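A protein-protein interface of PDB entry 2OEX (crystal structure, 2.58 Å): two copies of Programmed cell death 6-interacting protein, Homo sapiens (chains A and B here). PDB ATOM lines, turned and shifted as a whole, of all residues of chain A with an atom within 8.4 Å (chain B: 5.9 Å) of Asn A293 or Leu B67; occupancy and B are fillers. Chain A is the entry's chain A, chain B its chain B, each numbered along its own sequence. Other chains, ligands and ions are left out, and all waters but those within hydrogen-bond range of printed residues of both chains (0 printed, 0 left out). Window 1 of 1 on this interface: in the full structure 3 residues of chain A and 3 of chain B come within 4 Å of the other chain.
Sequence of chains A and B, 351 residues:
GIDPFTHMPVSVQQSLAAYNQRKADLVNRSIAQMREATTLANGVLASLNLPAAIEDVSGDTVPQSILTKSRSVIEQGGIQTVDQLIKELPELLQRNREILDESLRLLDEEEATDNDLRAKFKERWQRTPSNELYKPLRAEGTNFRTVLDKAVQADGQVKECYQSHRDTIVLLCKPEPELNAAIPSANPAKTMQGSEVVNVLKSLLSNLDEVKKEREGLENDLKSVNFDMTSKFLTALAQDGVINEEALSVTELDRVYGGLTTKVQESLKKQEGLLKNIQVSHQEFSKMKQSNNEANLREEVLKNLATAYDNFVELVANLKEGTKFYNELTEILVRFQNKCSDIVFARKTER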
ATOM      1  N   PRO A 184      37.523   4.165  -3.905  1.00  0.00           N
ATOM      2  CA  PRO A 184      36.162   4.660  -4.090  1.00  0.00           C
ATOM      3  C   PRO A 184      36.150   6.171  -4.038  1.00  0.00           C
ATOM      4  O   PRO A 184      36.863   6.772  -3.214  1.00  0.00           O
ATOM      5  CB  PRO A 184      35.408   4.073  -2.894  1.00  0.00           C
ATOM      6  CG  PRO A 184      36.107   2.779  -2.647  1.00  0.00           C
ATOM      7  CD  PRO A 184      37.566   3.045  -2.945  1.00  0.00           C
ATOM      8  N   SER A 185      35.377   6.777  -4.937  1.00  0.00           N
ATOM      9  CA  SER A 185      35.229   8.226  -4.944  1.00  0.00           C
ATOM     10  C   SER A 185      34.117   8.583  -3.970  1.00  0.00           C
ATOM     11  O   SER A 185      33.248   7.758  -3.679  1.00  0.00           O
ATOM     12  CB  SER A 185      34.965   8.770  -6.352  1.00  0.00           C
ATOM     13  OG  SER A 185      33.753   8.287  -6.891  1.00  0.00           O
ATOM     14  N   ALA A 186      34.167   9.798  -3.442  1.00  0.00           N
ATOM     15  CA  ALA A 186      33.174  10.232  -2.489  1.00  0.00           C
ATOM     16  C   ALA A 186      33.043  11.730  -2.536  1.00  0.00           C
ATOM     17  O   ALA A 186      33.696  12.390  -3.334  1.00  0.00           O
ATOM     18  CB  ALA A 186      33.547   9.770  -1.070  1.00  0.00           C
ATOM     19  N   GLN A 290      32.880  13.795   6.008  1.00  0.00           N
ATOM     20  CA  GLN A 290      31.676  13.110   5.575  1.00  0.00           C
ATOM     21  C   GLN A 290      31.468  11.761   6.251  1.00  0.00           C
ATOM     22  O   GLN A 290      32.424  11.023   6.520  1.00  0.00           O
ATOM     23  CB  GLN A 290      31.721  12.914   4.062  1.00  0.00           C
ATOM     24  CG  GLN A 290      32.058  14.168   3.267  1.00  0.00           C
ATOM     25  CD  GLN A 290      31.097  15.334   3.522  1.00  0.00           C
ATOM     26  OE1 GLN A 290      29.914  15.141   3.839  1.00  0.00           O
ATOM     27  NE2 GLN A 290      31.611  16.554   3.371  1.00  0.00           N
ATOM     28  N   SER A 291      30.210  11.437   6.525  1.00  0.00           N
ATOM     29  CA  SER A 291      29.877  10.087   6.939  1.00  0.00           C
ATOM     30  C   SER A 291      28.926   9.406   5.956  1.00  0.00           C
ATOM     31  O   SER A 291      28.166   8.511   6.343  1.00  0.00           O
ATOM     32  CB  SER A 291      29.308  10.065   8.356  1.00  0.00           C
ATOM     33  OG  SER A 291      29.126   8.723   8.778  1.00  0.00           O
ATOM     34  N   ASN A 292      28.954   9.818   4.684  1.00  0.00           N
ATOM     35  CA  ASN A 292      28.278   9.042   3.650  1.00  0.00           C
ATOM     36  C   ASN A 292      28.840   7.629   3.730  1.00  0.00           C
ATOM     37  O   ASN A 292      29.979   7.438   4.146  1.00  0.00           O
ATOM     38  CB  ASN A 292      28.566   9.578   2.245  1.00  0.00           C
ATOM     39  CG  ASN A 292      28.163  11.034   2.054  1.00  0.00           C
ATOM     40  OD1 ASN A 292      28.891  11.796   1.410  1.00  0.00           O
ATOM     41  ND2 ASN A 292      27.003  11.425   2.581  1.00  0.00           N
ATOM     42  N   ASN A 293      28.051   6.641   3.330  1.00  0.00           N
ATOM     43  CA  ASN A 293      28.549   5.279   3.260  1.00  0.00           C
ATOM     44  C   ASN A 293      29.800   5.186   2.387  1.00  0.00           C
ATOM     45  O   ASN A 293      30.703   4.411   2.675  1.00  0.00           O
ATOM     46  CB  ASN A 293      27.469   4.345   2.736  1.00  0.00           C
ATOM     47  CG  ASN A 293      27.726   2.907   3.094  1.00  0.00           C
ATOM     48  OD1 ASN A 293      27.288   2.431   4.154  1.00  0.00           O
ATOM     49  ND2 ASN A 293      28.446   2.201   2.227  1.00  0.00           N
ATOM     50  N   GLU A 294      29.848   6.003   1.339  1.00  0.00           N
ATOM     51  CA  GLU A 294      30.958   6.004   0.397  1.00  0.00           C
ATOM     52  C   GLU A 294      32.191   6.765   0.896  1.00  0.00           C
ATOM     53  O   GLU A 294      33.289   6.569   0.396  1.00  0.00           O
ATOM     54  CB  GLU A 294      30.500   6.509  -0.982  1.00  0.00           C
ATOM     55  CG  GLU A 294      29.243   7.378  -0.986  1.00  0.00           C
ATOM     56  CD  GLU A 294      27.937   6.573  -0.886  1.00  0.00           C
ATOM     57  OE1 GLU A 294      27.640   5.778  -1.808  1.00  0.00           O
ATOM     58  OE2 GLU A 294      27.197   6.751   0.109  1.00  0.00           O
ATOM     59  N   ALA A 295      31.999   7.634   1.881  1.00  0.00           N
ATOM     60  CA  ALA A 295      33.102   8.346   2.504  1.00  0.00           C
ATOM     61  C   ALA A 295      33.899   7.384   3.362  1.00  0.00           C
ATOM     62  O   ALA A 295      35.113   7.535   3.508  1.00  0.00           O
ATOM     63  CB  ALA A 295      32.586   9.484   3.341  1.00  0.00           C
ATOM     64  N   ASN A 296      33.208   6.395   3.930  1.00  0.00           N
ATOM     65  CA  ASN A 296      33.852   5.406   4.784  1.00  0.00           C
ATOM     66  C   ASN A 296      34.638   4.409   3.954  1.00  0.00           C
ATOM     67  O   ASN A 296      35.795   4.084   4.290  1.00  0.00           O
ATOM     68  CB  ASN A 296      32.836   4.718   5.709  1.00  0.00           C
ATOM     69  CG  ASN A 296      32.318   5.659   6.816  1.00  0.00           C
ATOM     70  OD1 ASN A 296      32.999   6.623   7.200  1.00  0.00           O
ATOM     71  ND2 ASN A 296      31.109   5.384   7.319  1.00  0.00           N
ATOM     72  N   LEU A 297      34.024   3.954   2.859  1.00  0.00           N
ATOM     73  CA  LEU A 297      34.691   3.091   1.903  1.00  0.00           C
ATOM     74  C   LEU A 297      35.984   3.705   1.421  1.00  0.00           C
ATOM     75  O   LEU A 297      37.018   3.038   1.453  1.00  0.00           O
ATOM     76  CB  LEU A 297      33.795   2.776   0.713  1.00  0.00           C
ATOM     77  CG  LEU A 297      32.640   1.795   0.935  1.00  0.00           C
ATOM     78  CD1 LEU A 297      31.758   1.750  -0.316  1.00  0.00           C
ATOM     79  CD2 LEU A 297      33.147   0.400   1.303  1.00  0.00           C
ATOM     80  N   ARG A 298      35.935   4.975   1.009  1.00  0.00           N
ATOM     81  CA  ARG A 298      37.141   5.697   0.589  1.00  0.00           C
ATOM     82  C   ARG A 298      38.153   5.830   1.716  1.00  0.00           C
ATOM     83  O   ARG A 298      39.345   5.778   1.469  1.00  0.00           O
ATOM     84  CB  ARG A 298      36.808   7.070   0.013  1.00  0.00           C
ATOM     85  CG  ARG A 298      38.022   7.922  -0.405  1.00  0.00           C
ATOM     86  CD  ARG A 298      37.569   9.242  -1.061  1.00  0.00           C
ATOM     87  NE  ARG A 298      38.661  10.041  -1.641  1.00  0.00           N
ATOM     88  CZ  ARG A 298      39.275   9.773  -2.797  1.00  0.00           C
ATOM     89  NH1 ARG A 298      38.914   8.715  -3.500  1.00  0.00           N
ATOM     90  NH2 ARG A 298      40.251  10.555  -3.251  1.00  0.00           N
ATOM     91  N   GLU A 299      37.686   5.998   2.947  1.00  0.00           N
ATOM     92  CA  GLU A 299      38.592   6.168   4.076  1.00  0.00           C
ATOM     93  C   GLU A 299      39.312   4.873   4.407  1.00  0.00           C
ATOM     94  O   GLU A 299      40.523   4.881   4.565  1.00  0.00           O
ATOM     95  CB  GLU A 299      37.877   6.727   5.310  1.00  0.00           C
ATOM     96  CG  GLU A 299      38.830   7.036   6.474  1.00  0.00           C
ATOM     97  CD  GLU A 299      38.326   8.118   7.428  1.00  0.00           C
ATOM     98  OE1 GLU A 299      38.740   9.299   7.277  1.00  0.00           O
ATOM     99  OE2 GLU A 299      37.526   7.789   8.330  1.00  0.00           O
ATOM    100  N   GLU A 300      38.578   3.764   4.490  1.00  0.00           N
ATOM    101  CA  GLU A 300      39.178   2.454   4.744  1.00  0.00           C
ATOM    102  C   GLU A 300      40.279   2.153   3.758  1.00  0.00           C
ATOM    103  O   GLU A 300      41.374   1.723   4.144  1.00  0.00           O
ATOM    104  CB  GLU A 300      38.142   1.345   4.624  1.00  0.00           C
ATOM    105  CG  GLU A 300      37.329   1.072   5.872  1.00  0.00           C
ATOM    106  CD  GLU A 300      36.113   0.182   5.595  1.00  0.00           C
ATOM    107  OE1 GLU A 300      35.862  -0.197   4.408  1.00  0.00           O
ATOM    108  OE2 GLU A 300      35.397  -0.133   6.579  1.00  0.00           O
ATOM    109  N   VAL B  62      19.378  -0.709   4.972  1.00  0.00           N
ATOM    110  CA  VAL B  62      20.243  -1.319   5.992  1.00  0.00           C
ATOM    111  C   VAL B  62      21.157  -0.254   6.583  1.00  0.00           C
ATOM    112  O   VAL B  62      21.977   0.312   5.846  1.00  0.00           O
ATOM    113  CB  VAL B  62      21.192  -2.408   5.439  1.00  0.00           C
ATOM    114  CG1 VAL B  62      21.669  -3.308   6.575  1.00  0.00           C
ATOM    115  CG2 VAL B  62      20.551  -3.221   4.329  1.00  0.00           C
ATOM    116  N   PRO B  63      21.052  -0.011   7.910  1.00  0.00           N
ATOM    117  CA  PRO B  63      21.857   0.974   8.611  1.00  0.00           C
ATOM    118  C   PRO B  63      23.331   0.812   8.285  1.00  0.00           C
ATOM    119  O   PRO B  63      23.839  -0.313   8.234  1.00  0.00           O
ATOM    120  CB  PRO B  63      21.614   0.629  10.084  1.00  0.00           C
ATOM    121  CG  PRO B  63      20.263   0.076  10.105  1.00  0.00           C
ATOM    122  CD  PRO B  63      20.148  -0.718   8.836  1.00  0.00           C
ATOM    123  N   GLN B  64      23.998   1.939   8.065  1.00  0.00           N
ATOM    124  CA  GLN B  64      25.398   1.979   7.656  1.00  0.00           C
ATOM    125  C   GLN B  64      26.234   1.031   8.507  1.00  0.00           C
ATOM    126  O   GLN B  64      26.872   0.123   7.974  1.00  0.00           O
ATOM    127  CB  GLN B  64      25.943   3.414   7.727  1.00  0.00           C
ATOM    128  CG  GLN B  64      24.855   4.505   7.533  1.00  0.00           C
ATOM    129  CD  GLN B  64      25.377   5.930   7.693  1.00  0.00           C
ATOM    130  OE1 GLN B  64      26.495   6.249   7.267  1.00  0.00           O
ATOM    131  NE2 GLN B  64      24.559   6.800   8.292  1.00  0.00           N
ATOM    132  N   SER B  65      26.189   1.214   9.830  1.00  0.00           N
ATOM    133  CA  SER B  65      27.034   0.456  10.742  1.00  0.00           C
ATOM    134  C   SER B  65      26.809  -1.062  10.675  1.00  0.00           C
ATOM    135  O   SER B  65      27.772  -1.835  10.861  1.00  0.00           O
ATOM    136  CB  SER B  65      26.854   0.944  12.171  1.00  0.00           C
ATOM    137  OG  SER B  65      25.571   0.582  12.637  1.00  0.00           O
ATOM    138  N   ILE B  66      25.562  -1.479  10.411  1.00  0.00           N
ATOM    139  CA  ILE B  66      25.249  -2.900  10.179  1.00  0.00           C
ATOM    140  C   ILE B  66      25.852  -3.352   8.844  1.00  0.00           C
ATOM    141  O   ILE B  66      26.450  -4.429   8.749  1.00  0.00           O
ATOM    142  CB  ILE B  66      23.743  -3.192  10.220  1.00  0.00           C
ATOM    143  CG1 ILE B  66      23.190  -2.937  11.628  1.00  0.00           C
ATOM    144  CG2 ILE B  66      23.450  -4.599   9.749  1.00  0.00           C
ATOM    145  CD1 ILE B  66      22.952  -4.149  12.531  1.00  0.00           C
ATOM    146  N   LEU B  67      25.739  -2.511   7.825  1.00  0.00           N
ATOM    147  CA  LEU B  67      26.310  -2.845   6.528  1.00  0.00           C
ATOM    148  C   LEU B  67      27.832  -2.910   6.610  1.00  0.00           C
ATOM    149  O   LEU B  67      28.457  -3.785   6.012  1.00  0.00           O
ATOM    150  CB  LEU B  67      25.849  -1.844   5.477  1.00  0.00           C
ATOM    151  CG  LEU B  67      26.152  -2.154   4.015  1.00  0.00           C
ATOM    152  CD1 LEU B  67      25.562  -3.492   3.560  1.00  0.00           C
ATOM    153  CD2 LEU B  67      25.653  -1.018   3.144  1.00  0.00           C
ATOM    154  N   THR B  68      28.423  -1.994   7.370  1.00  0.00           N
ATOM    155  CA  THR B  68      29.867  -1.993   7.621  1.00  0.00           C
ATOM    156  C   THR B  68      30.342  -3.245   8.377  1.00  0.00           C
ATOM    157  O   THR B  68      31.386  -3.831   8.028  1.00  0.00           O
ATOM    158  CB  THR B  68      30.282  -0.743   8.388  1.00  0.00           C
ATOM    159  OG1 THR B  68      30.356   0.352   7.472  1.00  0.00           O
ATOM    160  CG2 THR B  68      31.632  -0.933   9.096  1.00  0.00           C
ATOM    161  N   LYS B  69      29.587  -3.654   9.395  1.00  0.00           N
ATOM    162  CA  LYS B  69      29.883  -4.902  10.087  1.00  0.00           C
ATOM    163  C   LYS B  69      29.814  -6.055   9.094  1.00  0.00           C
ATOM    164  O   LYS B  69      30.641  -6.961   9.127  1.00  0.00           O
ATOM    165  CB  LYS B  69      28.925  -5.122  11.262  1.00  0.00           C
ATOM    166  CG  LYS B  69      29.256  -4.285  12.513  1.00  0.00           C
ATOM    167  CD  LYS B  69      28.031  -4.140  13.409  1.00  0.00           C
ATOM    168  CE  LYS B  69      28.387  -3.801  14.849  1.00  0.00           C
ATOM    169  NZ  LYS B  69      28.537  -2.357  15.206  1.00  0.00           N
ATOM    170  N   SER B  70      28.840  -5.989   8.192  1.00  0.00           N
ATOM    171  CA  SER B  70      28.679  -6.966   7.132  1.00  0.00           C
ATOM    172  C   SER B  70      29.889  -6.992   6.178  1.00  0.00           C
ATOM    173  O   SER B  70      30.276  -8.053   5.703  1.00  0.00           O
ATOM    174  CB  SER B  70      27.383  -6.682   6.380  1.00  0.00           C
ATOM    175  OG  SER B  70      27.169  -7.622   5.354  1.00  0.00           O
ATOM    176  N   ARG B  71      30.493  -5.833   5.917  1.00  0.00           N
ATOM    177  CA  ARG B  71      31.725  -5.773   5.114  1.00  0.00           C
ATOM    178  C   ARG B  71      32.807  -6.603   5.750  1.00  0.00           C
ATOM    179  O   ARG B  71      33.511  -7.333   5.051  1.00  0.00           O
ATOM    180  CB  ARG B  71      32.286  -4.357   5.022  1.00  0.00           C
ATOM    181  CG  ARG B  71      31.333  -3.324   4.518  1.00  0.00           C
ATOM    182  CD  ARG B  71      31.374  -3.215   3.020  1.00  0.00           C
ATOM    183  NE  ARG B  71      30.583  -2.065   2.606  1.00  0.00           N
ATOM    184  CZ  ARG B  71      29.282  -2.097   2.326  1.00  0.00           C
ATOM    185  NH1 ARG B  71      28.607  -3.244   2.396  1.00  0.00           N
ATOM    186  NH2 ARG B  71      28.663  -0.975   1.964  1.00  0.00           N
ATOM    187  N   SER B  72      32.960  -6.454   7.070  1.00  0.00           N
ATOM    188  CA  SER B  72      34.018  -7.130   7.803  1.00  0.00           C
ATOM    189  C   SER B  72      33.862  -8.642   7.740  1.00  0.00           C
ATOM    190  O   SER B  72      34.828  -9.362   7.501  1.00  0.00           O
ATOM    191  CB  SER B  72      34.077  -6.652   9.259  1.00  0.00           C
ATOM    192  OG  SER B  72      35.165  -5.769   9.473  1.00  0.00           O
ATOM    193  N   PRO B 175      24.894 -10.049   0.106  1.00  0.00           N
ATOM    194  CA  PRO B 175      25.045  -8.695  -0.440  1.00  0.00           C
ATOM    195  C   PRO B 175      23.983  -7.739   0.108  1.00  0.00           C
ATOM    196  O   PRO B 175      22.955  -8.190   0.620  1.00  0.00           O
ATOM    197  CB  PRO B 175      24.834  -8.900  -1.945  1.00  0.00           C
ATOM    198  CG  PRO B 175      24.039 -10.178  -2.049  1.00  0.00           C
ATOM    199  CD  PRO B 175      24.586 -11.032  -0.948  1.00  0.00           C
ATOM    200  N   GLU B 176      24.233  -6.436  -0.016  1.00  0.00           N
ATOM    201  CA  GLU B 176      23.332  -5.408   0.512  1.00  0.00           C
ATOM    202  C   GLU B 176      21.860  -5.642   0.162  1.00  0.00           C
ATOM    203  O   GLU B 176      21.053  -5.791   1.077  1.00  0.00           O
ATOM    204  CB  GLU B 176      23.779  -3.996   0.111  1.00  0.00           C
ATOM    205  CG  GLU B 176      22.829  -2.895   0.579  1.00  0.00           C
ATOM    206  CD  GLU B 176      23.424  -1.495   0.487  1.00  0.00           C
ATOM    207  OE1 GLU B 176      24.568  -1.350  -0.006  1.00  0.00           O
ATOM    208  OE2 GLU B 176      22.743  -0.533   0.919  1.00  0.00           O
ATOM    209  N   LEU B 179      20.371  -8.699   1.890  1.00  0.00           N
ATOM    210  CA  LEU B 179      20.425  -8.523   3.346  1.00  0.00           C
ATOM    211  C   LEU B 179      19.267  -7.669   3.847  1.00  0.00           C
ATOM    212  O   LEU B 179      18.700  -7.942   4.908  1.00  0.00           O
ATOM    213  CB  LEU B 179      21.771  -7.906   3.770  1.00  0.00           C
ATOM    214  CG  LEU B 179      22.002  -7.437   5.217  1.00  0.00           C
ATOM    215  CD1 LEU B 179      21.927  -8.586   6.225  1.00  0.00           C
ATOM    216  CD2 LEU B 179      23.327  -6.691   5.364  1.00  0.00           C
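No position is printed for both chains. Of the 5 pairs that touch across the chains among the printed residues, none has its exchanged pair printed and touching as well.
Printed residues of chain B within 4 Å of Ser A291: Gln B64 (3.0 Å). Asn A293 touches just these residues of chain B: Gln B64, Leu B67 and Arg B71. Printed residues of chain B within 4 Å of Leu A297: Arg B71 (3.8 Å). Printed residues of chain A within 4 Å of Gln B64: Ser A291 and Asn A293. Leu B67 touches just one residue of chain A: Asn A293. Of the printed residues of chain A, Arg B71 touches Asn A293 and Leu A297.
Asn A293 touches Gln B64. Leu B67 touches Asn A293 (CD2 to OD1, 3.9 Å). Arg B71 touches Leu A297 (NE to CD2, 3.8 Å).
Printed residues of chain A that touch a printed residue of chain B: Ser A291, Asn A293 and Leu A297. Hydrophobic or aromatic side chains of chain A that line the printed part of chain B: Leu A297. Of the 14 printed residues of chain B, 3 touch a printed residue of chain A. Among the printed residues, no Asp or Glu carboxylate lies within 4 Å of a Lys or Arg side-chain nitrogen of the other chain.
The backbone carbonyl oxygen (O) of Ser A291 lies close to the side-chain amide oxygen (OE1) of Gln B64, at 3.0 Å. The side-chain amide nitrogen of Asn A293 lies close to the guanidinium group of Arg B71 (3.2 Å).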
